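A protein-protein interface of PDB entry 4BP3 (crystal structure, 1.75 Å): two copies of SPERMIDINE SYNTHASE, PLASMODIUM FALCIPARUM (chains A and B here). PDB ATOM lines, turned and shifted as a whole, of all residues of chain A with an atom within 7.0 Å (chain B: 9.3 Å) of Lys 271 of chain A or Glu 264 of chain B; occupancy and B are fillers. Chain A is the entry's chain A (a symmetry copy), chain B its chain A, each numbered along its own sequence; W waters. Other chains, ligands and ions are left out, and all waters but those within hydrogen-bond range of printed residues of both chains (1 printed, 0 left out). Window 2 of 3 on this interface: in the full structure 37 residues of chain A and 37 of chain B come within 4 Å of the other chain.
Of the 13 printed residues of chain A, 5 touch a printed residue of chain B. Hydrophobic or aromatic side chains of chain A within 4 Å of the printed part of chain B: Ala 268, Pro 273 and Leu 277. Of the 22 printed residues of chain B, 6 touch a printed residue of chain A. Printed residues of chain B that touch a printed residue of chain A: Tyr 260, Asn 262, Glu 264, Asn 265, Ala 268 and Lys 271. Hydrophobic or aromatic side chains of chain B that line the printed part of chain A: Tyr 260 and Ala 268. Among the printed residues, Asp or Glu carboxylates within 4 Å of a Lys or Arg side-chain nitrogen of the other chain: Lys 271 of chain A with Glu 264 of chain B.
OH of Tyr 260 of chain B is in hydrogen-bond range of N of Ser 222 of chain B (3.2 Å). The side-chain amide nitrogen of Asn 265 of chain B sits at hydrogen-bond distance from the backbone carbonyl oxygen of Tyr 260 of chain B (2.9 Å). The backbone NH (N) of Glu 264 of chain B lies close to the side-chain amide oxygen (OD1) of Asn 262 of chain B. OD1 of Asn 262 of chain B lies within hydrogen-bond range of N of Asn 265 of chain B (3.0 Å).
Ala 268 of chain B touches its own counterpart, Ala 268 of chain A. Ala 268 of chain A touches Lys 271 of chain B, and with the chains exchanged Lys 271 of chain A touches Ala 268 of chain B. 8 positions are printed for both chains. Of the 10 pairs that touch across the chains among the printed residues, 3 have their exchanged pair printed and touching as well.
O of Ala 268 of chain A touches CB of Ala 268 of chain B, at 3.8 Å. Ala 268 of chain A touches Lys 271 of chain B. Lys 271 of chain A touches Asn 265 of chain B (O to CB, 3.7 Å). Lys 271 of chain A touches Ala 268 of chain B. Leu 272 of chain A touches Asn 262 of chain B. Pro 273 of chain A touches Tyr 260 of chain B (CA to O, 3.8 Å). Pro 273 of chain A touches Asn 265 of chain B (CA to ND2, 3.7 Å). Asn 262 of chain B touches Leu 277 of chain A.
Water W1 lies within hydrogen-bond range of the backbone carbonyl oxygen of Leu 272 of chain A (2.9 Å), the side-chain amide oxygen of Asn 262 of chain B (3.0 Å) and the side-chain amide nitrogen of Asn 265 of chain B (3.4 Å).
The side-chain carboxylate (OE1) of Glu 264 of chain B is in salt-bridge range of the side-chain amino group (NZ) of Lys 271 of chain A (3.4 Å). ND2 of Asn 265 of chain B lies within hydrogen-bond range of O of Leu 272 of chain A (2.8 Å).
Of the printed residues of chain A, Asn 265 of chain B touches Lys 271 (3.7 Å), Leu 272 (2.8 Å) and Pro 273 (3.7 Å). Of the printed residues of chain A, Tyr 260 of chain B touches Pro 273. Of the printed residues of chain B, Pro 273 of chain A touches Tyr 260 and Asn 265. Lys 248 of chain B touches none of the printed residues of chain A. The nearest printed residue of chain A that does not touch Ala 268 of chain B is Ala 269 of chain A (5.7 Å).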
ATOM      1  N   TYR A 218     -26.423 -18.344  -7.252  1.00  0.00           N
ATOM      2  CA  TYR A 218     -25.041 -17.901  -7.178  1.00  0.00           C
ATOM      3  C   TYR A 218     -24.989 -16.643  -7.992  1.00  0.00           C
ATOM      4  O   TYR A 218     -25.550 -16.617  -9.095  1.00  0.00           O
ATOM      5  CB  TYR A 218     -24.176 -18.986  -7.700  1.00  0.00           C
ATOM      6  CG  TYR A 218     -22.707 -18.722  -7.581  1.00  0.00           C
ATOM      7  CD1 TYR A 218     -22.008 -17.987  -8.560  1.00  0.00           C
ATOM      8  CD2 TYR A 218     -22.018 -19.246  -6.547  1.00  0.00           C
ATOM      9  CE1 TYR A 218     -20.598 -17.755  -8.407  1.00  0.00           C
ATOM     10  CE2 TYR A 218     -20.652 -19.042  -6.395  1.00  0.00           C
ATOM     11  CZ  TYR A 218     -19.949 -18.306  -7.336  1.00  0.00           C
ATOM     12  OH  TYR A 218     -18.593 -18.150  -7.131  1.00  0.00           O
ATOM     13  N   ALA A 219     -24.378 -15.583  -7.445  1.00  0.00           N
ATOM     14  CA  ALA A 219     -24.291 -14.313  -8.042  1.00  0.00           C
ATOM     15  C   ALA A 219     -22.831 -13.976  -8.137  1.00  0.00           C
ATOM     16  O   ALA A 219     -22.020 -14.536  -7.410  1.00  0.00           O
ATOM     17  CB  ALA A 219     -24.960 -13.281  -7.201  1.00  0.00           C
ATOM     18  N   ASN A 220     -22.486 -13.012  -8.978  1.00  0.00           N
ATOM     19  CA  ASN A 220     -21.064 -12.746  -9.155  1.00  0.00           C
ATOM     20  C   ASN A 220     -20.880 -11.240  -9.014  1.00  0.00           C
ATOM     21  O   ASN A 220     -21.699 -10.451  -9.442  1.00  0.00           O
ATOM     22  CB  ASN A 220     -20.539 -13.342 -10.491  1.00  0.00           C
ATOM     23  CG  ASN A 220     -19.021 -13.307 -10.585  1.00  0.00           C
ATOM     24  OD1 ASN A 220     -18.311 -13.638  -9.665  1.00  0.00           O
ATOM     25  ND2 ASN A 220     -18.538 -12.911 -11.710  1.00  0.00           N
ATOM     26  N   THR A 244     -32.902 -13.246  -6.237  1.00  0.00           N
ATOM     27  CA  THR A 244     -32.577 -12.504  -7.484  1.00  0.00           C
ATOM     28  C   THR A 244     -33.345 -11.216  -7.686  1.00  0.00           C
ATOM     29  O   THR A 244     -32.877 -10.326  -8.446  1.00  0.00           O
ATOM     30  CB  THR A 244     -32.651 -13.392  -8.756  1.00  0.00           C
ATOM     31  OG1 THR A 244     -33.997 -13.793  -8.968  1.00  0.00           O
ATOM     32  CG2 THR A 244     -31.838 -14.666  -8.581  1.00  0.00           C
ATOM     33  N   HIS A 266     -28.498  -5.608  -8.930  1.00  0.00           N
ATOM     34  CA  HIS A 266     -28.907  -6.736  -8.103  1.00  0.00           C
ATOM     35  C   HIS A 266     -29.283  -8.027  -8.871  1.00  0.00           C
ATOM     36  O   HIS A 266     -28.765  -9.141  -8.622  1.00  0.00           O
ATOM     37  CB  HIS A 266     -30.084  -6.241  -7.247  1.00  0.00           C
ATOM     38  CG  HIS A 266     -30.644  -7.259  -6.317  1.00  0.00           C
ATOM     39  ND1 HIS A 266     -31.165  -6.903  -5.075  1.00  0.00           N
ATOM     40  CD2 HIS A 266     -30.757  -8.607  -6.395  1.00  0.00           C
ATOM     41  CE1 HIS A 266     -31.580  -7.995  -4.455  1.00  0.00           C
ATOM     42  NE2 HIS A 266     -31.388  -9.037  -5.242  1.00  0.00           N
ATOM     43  N   SER A 267     -30.248  -7.970  -9.801  1.00  0.00           N
ATOM     44  CA  SER A 267     -30.616  -9.199 -10.501  1.00  0.00           C
ATOM     45  C   SER A 267     -29.569  -9.566 -11.571  1.00  0.00           C
ATOM     46  O   SER A 267     -29.430 -10.697 -11.884  1.00  0.00           O
ATOM     47  CB  SER A 267     -32.015  -9.054 -11.112  1.00  0.00           C
ATOM     48  OG  SER A 267     -32.908  -8.494 -10.135  1.00  0.00           O
ATOM     49  N   ALA A 268     -28.866  -8.577 -12.086  1.00  0.00           N
ATOM     50  CA  ALA A 268     -27.858  -8.872 -13.126  1.00  0.00           C
ATOM     51  C   ALA A 268     -26.769  -9.825 -12.639  1.00  0.00           C
ATOM     52  O   ALA A 268     -26.229 -10.737 -13.341  1.00  0.00           O
ATOM     53  CB  ALA A 268     -27.290  -7.585 -13.637  1.00  0.00           C
ATOM     54  N   ALA A 269     -26.470  -9.697 -11.346  1.00  0.00           N
ATOM     55  CA  ALA A 269     -25.350 -10.377 -10.766  1.00  0.00           C
ATOM     56  C   ALA A 269     -25.570 -11.845 -10.852  1.00  0.00           C
ATOM     57  O   ALA A 269     -24.635 -12.634 -10.803  1.00  0.00           O
ATOM     58  CB  ALA A 269     -25.165  -9.895  -9.317  1.00  0.00           C
ATOM     59  N   PHE A 270     -26.838 -12.269 -11.020  1.00  0.00           N
ATOM     60  CA  PHE A 270     -27.151 -13.703 -11.054  1.00  0.00           C
ATOM     61  C   PHE A 270     -27.115 -14.347 -12.484  1.00  0.00           C
ATOM     62  O   PHE A 270     -27.276 -15.544 -12.644  1.00  0.00           O
ATOM     63  CB  PHE A 270     -28.531 -13.944 -10.446  1.00  0.00           C
ATOM     64  CG  PHE A 270     -28.559 -13.733  -8.941  1.00  0.00           C
ATOM     65  CD1 PHE A 270     -28.721 -12.489  -8.407  1.00  0.00           C
ATOM     66  CD2 PHE A 270     -28.340 -14.794  -8.120  1.00  0.00           C
ATOM     67  CE1 PHE A 270     -28.753 -12.303  -7.002  1.00  0.00           C
ATOM     68  CE2 PHE A 270     -28.343 -14.620  -6.718  1.00  0.00           C
ATOM     69  CZ  PHE A 270     -28.554 -13.378  -6.193  1.00  0.00           C
ATOM     70  N   LYS A 271     -26.814 -13.552 -13.480  1.00  0.00           N
ATOM     71  CA  LYS A 271     -26.777 -14.122 -14.866  1.00  0.00           C
ATOM     72  C   LYS A 271     -25.330 -14.590 -15.092  1.00  0.00           C
ATOM     73  O   LYS A 271     -24.510 -13.775 -15.297  1.00  0.00           O
ATOM     74  CB  LYS A 271     -27.168 -13.046 -15.837  1.00  0.00           C
ATOM     75  CG  LYS A 271     -28.499 -12.352 -15.519  1.00  0.00           C
ATOM     76  CD  LYS A 271     -29.519 -13.398 -15.193  1.00  0.00           C
ATOM     77  CE  LYS A 271     -30.939 -12.779 -15.332  1.00  0.00           C
ATOM     78  NZ  LYS A 271     -31.837 -13.952 -15.128  1.00  0.00           N
ATOM     79  N   LEU A 272     -25.072 -15.871 -15.029  1.00  0.00           N
ATOM     80  CA  LEU A 272     -23.743 -16.428 -14.959  1.00  0.00           C
ATOM     81  C   LEU A 272     -23.223 -16.953 -16.321  1.00  0.00           C
ATOM     82  O   LEU A 272     -23.991 -17.243 -17.228  1.00  0.00           O
ATOM     83  CB  LEU A 272     -23.758 -17.626 -14.055  1.00  0.00           C
ATOM     84  CG  LEU A 272     -24.227 -17.310 -12.608  1.00  0.00           C
ATOM     85  CD1 LEU A 272     -24.268 -18.673 -11.940  1.00  0.00           C
ATOM     86  CD2 LEU A 272     -23.254 -16.347 -12.002  1.00  0.00           C
ATOM     87  N   PRO A 273     -21.919 -17.159 -16.396  1.00  0.00           N
ATOM     88  CA  PRO A 273     -21.369 -17.690 -17.656  1.00  0.00           C
ATOM     89  C   PRO A 273     -21.822 -19.083 -17.976  1.00  0.00           C
ATOM     90  O   PRO A 273     -22.003 -19.951 -17.067  1.00  0.00           O
ATOM     91  CB  PRO A 273     -19.844 -17.656 -17.396  1.00  0.00           C
ATOM     92  CG  PRO A 273     -19.662 -16.453 -16.462  1.00  0.00           C
ATOM     93  CD  PRO A 273     -20.886 -16.539 -15.536  1.00  0.00           C
ATOM     94  N   LEU A 277     -23.042 -22.566 -15.514  1.00  0.00           N
ATOM     95  CA  LEU A 277     -24.398 -23.213 -15.593  1.00  0.00           C
ATOM     96  C   LEU A 277     -24.354 -24.623 -15.960  1.00  0.00           C
ATOM     97  O   LEU A 277     -25.053 -25.462 -15.377  1.00  0.00           O
ATOM     98  CB  LEU A 277     -25.309 -22.465 -16.544  1.00  0.00           C
ATOM     99  CG  LEU A 277     -25.546 -21.047 -16.132  1.00  0.00           C
ATOM    100  CD1 LEU A 277     -26.350 -20.341 -17.178  1.00  0.00           C
ATOM    101  CD2 LEU A 277     -26.303 -21.056 -14.785  1.00  0.00           C
ATOM    102  N   MET B  67     -18.304 -12.652 -25.901  1.00  0.00           N
ATOM    103  CA  MET B  67     -19.158 -11.482 -25.678  1.00  0.00           C
ATOM    104  C   MET B  67     -19.001 -10.376 -26.699  1.00  0.00           C
ATOM    105  O   MET B  67     -19.979  -9.761 -27.044  1.00  0.00           O
ATOM    106  CB  MET B  67     -19.031 -10.934 -24.238  1.00  0.00           C
ATOM    107  CG  MET B  67     -19.255 -12.033 -23.232  1.00  0.00           C
ATOM    108  SD  MET B  67     -20.999 -12.459 -23.009  1.00  0.00           S
ATOM    109  CE  MET B  67     -21.587 -10.795 -22.544  1.00  0.00           C
ATOM    110  N   VAL B  71     -22.705 -10.542 -28.649  1.00  0.00           N
ATOM    111  CA  VAL B  71     -23.532  -9.408 -28.333  1.00  0.00           C
ATOM    112  C   VAL B  71     -23.973  -8.712 -29.647  1.00  0.00           C
ATOM    113  O   VAL B  71     -25.184  -8.635 -29.937  1.00  0.00           O
ATOM    114  CB  VAL B  71     -22.843  -8.410 -27.404  1.00  0.00           C
ATOM    115  CG1 VAL B  71     -23.465  -7.050 -27.394  1.00  0.00           C
ATOM    116  CG2 VAL B  71     -22.757  -8.928 -25.995  1.00  0.00           C
ATOM    117  N   THR B  74     -25.979 -11.187 -32.386  1.00  0.00           N
ATOM    118  CA  THR B  74     -27.294 -11.655 -32.095  1.00  0.00           C
ATOM    119  C   THR B  74     -28.259 -10.501 -32.147  1.00  0.00           C
ATOM    120  O   THR B  74     -29.454 -10.723 -32.091  1.00  0.00           O
ATOM    121  CB  THR B  74     -27.387 -12.240 -30.674  1.00  0.00           C
ATOM    122  OG1 THR B  74     -26.968 -11.219 -29.734  1.00  0.00           O
ATOM    123  CG2 THR B  74     -26.632 -13.481 -30.564  1.00  0.00           C
ATOM    124  N   ASN B 220     -20.013  -4.903 -19.340  1.00  0.00           N
ATOM    125  CA  ASN B 220     -18.804  -5.273 -18.617  1.00  0.00           C
ATOM    126  C   ASN B 220     -18.694  -6.790 -18.696  1.00  0.00           C
ATOM    127  O   ASN B 220     -19.673  -7.508 -18.642  1.00  0.00           O
ATOM    128  CB  ASN B 220     -18.809  -4.698 -17.172  1.00  0.00           C
ATOM    129  CG  ASN B 220     -17.461  -4.846 -16.484  1.00  0.00           C
ATOM    130  OD1 ASN B 220     -16.420  -4.585 -17.040  1.00  0.00           O
ATOM    131  ND2 ASN B 220     -17.496  -5.261 -15.266  1.00  0.00           N
ATOM    132  N   SER B 222     -16.514 -10.296 -17.227  1.00  0.00           N
ATOM    133  CA  SER B 222     -15.600 -10.831 -16.274  1.00  0.00           C
ATOM    134  C   SER B 222     -14.600 -11.669 -17.099  1.00  0.00           C
ATOM    135  O   SER B 222     -14.960 -12.655 -17.824  1.00  0.00           O
ATOM    136  CB  SER B 222     -16.342 -11.709 -15.318  1.00  0.00           C
ATOM    137  OG  SER B 222     -15.507 -12.581 -14.610  1.00  0.00           O
ATOM    138  N   THR B 244     -28.432  -3.920 -25.990  1.00  0.00           N
ATOM    139  CA  THR B 244     -28.686  -4.665 -24.728  1.00  0.00           C
ATOM    140  C   THR B 244     -29.567  -5.889 -24.869  1.00  0.00           C
ATOM    141  O   THR B 244     -29.509  -6.799 -23.999  1.00  0.00           O
ATOM    142  CB  THR B 244     -29.192  -3.754 -23.577  1.00  0.00           C
ATOM    143  OG1 THR B 244     -30.477  -3.249 -23.911  1.00  0.00           O
ATOM    144  CG2 THR B 244     -28.282  -2.549 -23.394  1.00  0.00           C
ATOM    145  N   LYS B 245     -30.372  -5.974 -25.946  1.00  0.00           N
ATOM    146  CA  LYS B 245     -31.279  -7.120 -26.080  1.00  0.00           C
ATOM    147  C   LYS B 245     -31.034  -7.998 -27.330  1.00  0.00           C
ATOM    148  O   LYS B 245     -31.272  -7.565 -28.384  1.00  0.00           O
ATOM    149  CB  LYS B 245     -32.722  -6.583 -26.115  1.00  0.00           C
ATOM    150  CG  LYS B 245     -33.098  -5.871 -24.805  1.00  0.00           C
ATOM    151  CD  LYS B 245     -34.488  -5.218 -24.849  1.00  0.00           C
ATOM    152  CE  LYS B 245     -34.563  -4.046 -23.882  1.00  0.00           C
ATOM    153  NZ  LYS B 245     -35.966  -3.593 -23.663  1.00  0.00           N
ATOM    154  N   PRO B 246     -30.606  -9.235 -27.180  1.00  0.00           N
ATOM    155  CA  PRO B 246     -30.449 -10.048 -28.385  1.00  0.00           C
ATOM    156  C   PRO B 246     -31.771 -10.235 -29.164  1.00  0.00           C
ATOM    157  O   PRO B 246     -32.842 -10.357 -28.505  1.00  0.00           O
ATOM    158  CB  PRO B 246     -30.019 -11.414 -27.853  1.00  0.00           C
ATOM    159  CG  PRO B 246     -30.297 -11.371 -26.382  1.00  0.00           C
ATOM    160  CD  PRO B 246     -30.232  -9.950 -25.968  1.00  0.00           C
ATOM    161  N   LYS B 248     -31.935 -12.965 -31.399  1.00  0.00           N
ATOM    162  CA  LYS B 248     -31.997 -14.379 -31.649  1.00  0.00           C
ATOM    163  C   LYS B 248     -31.256 -15.090 -30.576  1.00  0.00           C
ATOM    164  O   LYS B 248     -30.468 -14.468 -29.837  1.00  0.00           O
ATOM    165  CB  LYS B 248     -31.281 -14.713 -32.970  1.00  0.00           C
ATOM    166  CG  LYS B 248     -29.762 -14.487 -32.973  1.00  0.00           C
ATOM    167  CD  LYS B 248     -29.132 -14.418 -34.395  1.00  0.00           C
ATOM    168  CE  LYS B 248     -29.583 -13.179 -35.179  1.00  0.00           C
ATOM    169  NZ  LYS B 248     -28.501 -12.528 -35.972  1.00  0.00           N
ATOM    170  N   LYS B 249     -31.457 -16.405 -30.571  1.00  0.00           N
ATOM    171  CA  LYS B 249     -30.727 -17.361 -29.778  1.00  0.00           C
ATOM    172  C   LYS B 249     -29.872 -18.283 -30.625  1.00  0.00           C
ATOM    173  O   LYS B 249     -30.209 -18.705 -31.722  1.00  0.00           O
ATOM    174  CB  LYS B 249     -31.721 -18.231 -29.011  1.00  0.00           C
ATOM    175  CG  LYS B 249     -32.781 -17.396 -28.295  1.00  0.00           C
ATOM    176  CD  LYS B 249     -33.408 -18.122 -27.098  1.00  0.00           C
ATOM    177  CE  LYS B 249     -34.329 -17.181 -26.309  1.00  0.00           C
ATOM    178  NZ  LYS B 249     -34.231 -17.430 -24.843  1.00  0.00           N
ATOM    179  N   TYR B 260     -19.326 -18.968 -22.460  1.00  0.00           N
ATOM    180  CA  TYR B 260     -19.670 -17.795 -21.674  1.00  0.00           C
ATOM    181  C   TYR B 260     -20.985 -17.198 -22.109  1.00  0.00           C
ATOM    182  O   TYR B 260     -21.922 -17.021 -21.311  1.00  0.00           O
ATOM    183  CB  TYR B 260     -18.589 -16.711 -21.771  1.00  0.00           C
ATOM    184  CG  TYR B 260     -18.669 -15.538 -20.777  1.00  0.00           C
ATOM    185  CD1 TYR B 260     -19.595 -14.548 -20.919  1.00  0.00           C
ATOM    186  CD2 TYR B 260     -17.721 -15.390 -19.711  1.00  0.00           C
ATOM    187  CE1 TYR B 260     -19.670 -13.449 -20.066  1.00  0.00           C
ATOM    188  CE2 TYR B 260     -17.759 -14.274 -18.879  1.00  0.00           C
ATOM    189  CZ  TYR B 260     -18.747 -13.312 -19.030  1.00  0.00           C
ATOM    190  OH  TYR B 260     -18.869 -12.155 -18.238  1.00  0.00           O
ATOM    191  N   TYR B 261     -21.091 -16.802 -23.354  1.00  0.00           N
ATOM    192  CA  TYR B 261     -22.253 -16.131 -23.808  1.00  0.00           C
ATOM    193  C   TYR B 261     -23.492 -17.005 -23.729  1.00  0.00           C
ATOM    194  O   TYR B 261     -23.469 -18.259 -23.978  1.00  0.00           O
ATOM    195  CB  TYR B 261     -22.090 -15.683 -25.290  1.00  0.00           C
ATOM    196  CG  TYR B 261     -23.264 -14.973 -25.795  1.00  0.00           C
ATOM    197  CD1 TYR B 261     -24.320 -15.675 -26.351  1.00  0.00           C
ATOM    198  CD2 TYR B 261     -23.313 -13.628 -25.784  1.00  0.00           C
ATOM    199  CE1 TYR B 261     -25.465 -15.023 -26.774  1.00  0.00           C
ATOM    200  CE2 TYR B 261     -24.407 -12.961 -26.206  1.00  0.00           C
ATOM    201  CZ  TYR B 261     -25.464 -13.676 -26.743  1.00  0.00           C
ATOM    202  OH  TYR B 261     -26.542 -12.985 -27.132  1.00  0.00           O
ATOM    203  N   ASN B 262     -24.541 -16.322 -23.301  1.00  0.00           N
ATOM    204  CA  ASN B 262     -25.942 -16.802 -23.550  1.00  0.00           C
ATOM    205  C   ASN B 262     -26.869 -15.653 -23.545  1.00  0.00           C
ATOM    206  O   ASN B 262     -26.492 -14.503 -23.344  1.00  0.00           O
ATOM    207  CB  ASN B 262     -26.382 -17.900 -22.569  1.00  0.00           C
ATOM    208  CG  ASN B 262     -26.334 -17.441 -21.109  1.00  0.00           C
ATOM    209  OD1 ASN B 262     -26.559 -16.297 -20.782  1.00  0.00           O
ATOM    210  ND2 ASN B 262     -25.975 -18.349 -20.250  1.00  0.00           N
ATOM    211  N   TYR B 263     -28.126 -15.946 -23.865  1.00  0.00           N
ATOM    212  CA  TYR B 263     -29.098 -14.935 -24.120  1.00  0.00           C
ATOM    213  C   TYR B 263     -29.280 -13.969 -22.891  1.00  0.00           C
ATOM    214  O   TYR B 263     -29.346 -12.732 -22.992  1.00  0.00           O
ATOM    215  CB  TYR B 263     -30.383 -15.716 -24.507  1.00  0.00           C
ATOM    216  CG  TYR B 263     -31.553 -14.839 -24.697  1.00  0.00           C
ATOM    217  CD1 TYR B 263     -32.346 -14.442 -23.614  1.00  0.00           C
ATOM    218  CD2 TYR B 263     -31.882 -14.378 -25.951  1.00  0.00           C
ATOM    219  CE1 TYR B 263     -33.419 -13.579 -23.800  1.00  0.00           C
ATOM    220  CE2 TYR B 263     -32.970 -13.542 -26.148  1.00  0.00           C
ATOM    221  CZ  TYR B 263     -33.727 -13.143 -25.072  1.00  0.00           C
ATOM    222  OH  TYR B 263     -34.776 -12.297 -25.320  1.00  0.00           O
ATOM    223  N   GLU B 264     -29.314 -14.519 -21.709  1.00  0.00           N
ATOM    224  CA  GLU B 264     -29.572 -13.653 -20.479  1.00  0.00           C
ATOM    225  C   GLU B 264     -28.353 -12.781 -20.067  1.00  0.00           C
ATOM    226  O   GLU B 264     -28.453 -11.579 -19.797  1.00  0.00           O
ATOM    227  CB  GLU B 264     -29.866 -14.619 -19.364  1.00  0.00           C
ATOM    228  CG  GLU B 264     -31.099 -15.408 -19.671  1.00  0.00           C
ATOM    229  CD  GLU B 264     -31.960 -15.533 -18.482  1.00  0.00           C
ATOM    230  OE1 GLU B 264     -31.645 -16.370 -17.571  1.00  0.00           O
ATOM    231  OE2 GLU B 264     -32.926 -14.756 -18.484  1.00  0.00           O
ATOM    232  N   ASN B 265     -27.169 -13.382 -20.167  1.00  0.00           N
ATOM    233  CA  ASN B 265     -25.999 -12.691 -19.632  1.00  0.00           C
ATOM    234  C   ASN B 265     -25.565 -11.675 -20.657  1.00  0.00           C
ATOM    235  O   ASN B 265     -24.971 -10.638 -20.346  1.00  0.00           O
ATOM    236  CB  ASN B 265     -24.987 -13.657 -18.950  1.00  0.00           C
ATOM    237  CG  ASN B 265     -24.240 -14.448 -19.910  1.00  0.00           C
ATOM    238  OD1 ASN B 265     -24.067 -13.978 -21.031  1.00  0.00           O
ATOM    239  ND2 ASN B 265     -23.801 -15.695 -19.516  1.00  0.00           N
ATOM    240  N   HIS B 266     -26.055 -11.828 -21.890  1.00  0.00           N
ATOM    241  CA  HIS B 266     -26.015 -10.685 -22.793  1.00  0.00           C
ATOM    242  C   HIS B 266     -26.566  -9.358 -22.217  1.00  0.00           C
ATOM    243  O   HIS B 266     -25.908  -8.290 -22.222  1.00  0.00           O
ATOM    244  CB  HIS B 266     -26.788 -11.103 -24.054  1.00  0.00           C
ATOM    245  CG  HIS B 266     -26.854 -10.060 -25.114  1.00  0.00           C
ATOM    246  ND1 HIS B 266     -26.864 -10.395 -26.466  1.00  0.00           N
ATOM    247  CD2 HIS B 266     -26.886  -8.706 -25.066  1.00  0.00           C
ATOM    248  CE1 HIS B 266     -26.914  -9.284 -27.183  1.00  0.00           C
ATOM    249  NE2 HIS B 266     -26.972  -8.248 -26.367  1.00  0.00           N
ATOM    250  N   SER B 267     -27.822  -9.327 -21.748  1.00  0.00           N
ATOM    251  CA  SER B 267     -28.344  -8.062 -21.234  1.00  0.00           C
ATOM    252  C   SER B 267     -27.783  -7.759 -19.829  1.00  0.00           C
ATOM    253  O   SER B 267     -27.694  -6.637 -19.470  1.00  0.00           O
ATOM    254  CB  SER B 267     -29.876  -8.091 -21.231  1.00  0.00           C
ATOM    255  OG  SER B 267     -30.347  -8.596 -22.491  1.00  0.00           O
ATOM    256  N   ALA B 268     -27.421  -8.790 -19.093  1.00  0.00           N
ATOM    257  CA  ALA B 268     -26.889  -8.556 -17.734  1.00  0.00           C
ATOM    258  C   ALA B 268     -25.628  -7.697 -17.733  1.00  0.00           C
ATOM    259  O   ALA B 268     -25.343  -6.817 -16.860  1.00  0.00           O
ATOM    260  CB  ALA B 268     -26.671  -9.875 -17.059  1.00  0.00           C
ATOM    261  N   ALA B 269     -24.850  -7.867 -18.802  1.00  0.00           N
ATOM    262  CA  ALA B 269     -23.543  -7.284 -18.878  1.00  0.00           C
ATOM    263  C   ALA B 269     -23.667  -5.802 -18.864  1.00  0.00           C
ATOM    264  O   ALA B 269     -22.733  -5.087 -18.525  1.00  0.00           O
ATOM    265  CB  ALA B 269     -22.835  -7.801 -20.143  1.00  0.00           C
ATOM    266  N   PHE B 270     -24.861  -5.281 -19.207  1.00  0.00           N
ATOM    267  CA  PHE B 270     -25.052  -3.826 -19.277  1.00  0.00           C
ATOM    268  C   PHE B 270     -25.538  -3.164 -17.941  1.00  0.00           C
ATOM    269  O   PHE B 270     -25.659  -1.956 -17.839  1.00  0.00           O
ATOM    270  CB  PHE B 270     -26.054  -3.490 -20.380  1.00  0.00           C
ATOM    271  CG  PHE B 270     -25.498  -3.723 -21.775  1.00  0.00           C
ATOM    272  CD1 PHE B 270     -25.529  -4.959 -22.349  1.00  0.00           C
ATOM    273  CD2 PHE B 270     -24.891  -2.695 -22.425  1.00  0.00           C
ATOM    274  CE1 PHE B 270     -25.013  -5.164 -23.655  1.00  0.00           C
ATOM    275  CE2 PHE B 270     -24.350  -2.890 -23.715  1.00  0.00           C
ATOM    276  CZ  PHE B 270     -24.428  -4.120 -24.300  1.00  0.00           C
ATOM    277  N   LYS B 271     -25.720  -3.965 -16.920  1.00  0.00           N
ATOM    278  CA  LYS B 271     -26.193  -3.377 -15.625  1.00  0.00           C
ATOM    279  C   LYS B 271     -24.924  -3.017 -14.835  1.00  0.00           C
ATOM    280  O   LYS B 271     -24.318  -3.889 -14.334  1.00  0.00           O
ATOM    281  CB  LYS B 271     -27.018  -4.405 -14.906  1.00  0.00           C
ATOM    282  CG  LYS B 271     -28.162  -5.000 -15.738  1.00  0.00           C
ATOM    283  CD  LYS B 271     -28.885  -3.885 -16.426  1.00  0.00           C
ATOM    284  CE  LYS B 271     -30.287  -4.392 -16.872  1.00  0.00           C
ATOM    285  NZ  LYS B 271     -30.937  -3.157 -17.398  1.00  0.00           N
HETATM  286  O   HOH W   1     -26.689 -16.453 -17.798  1.00  0.00           O
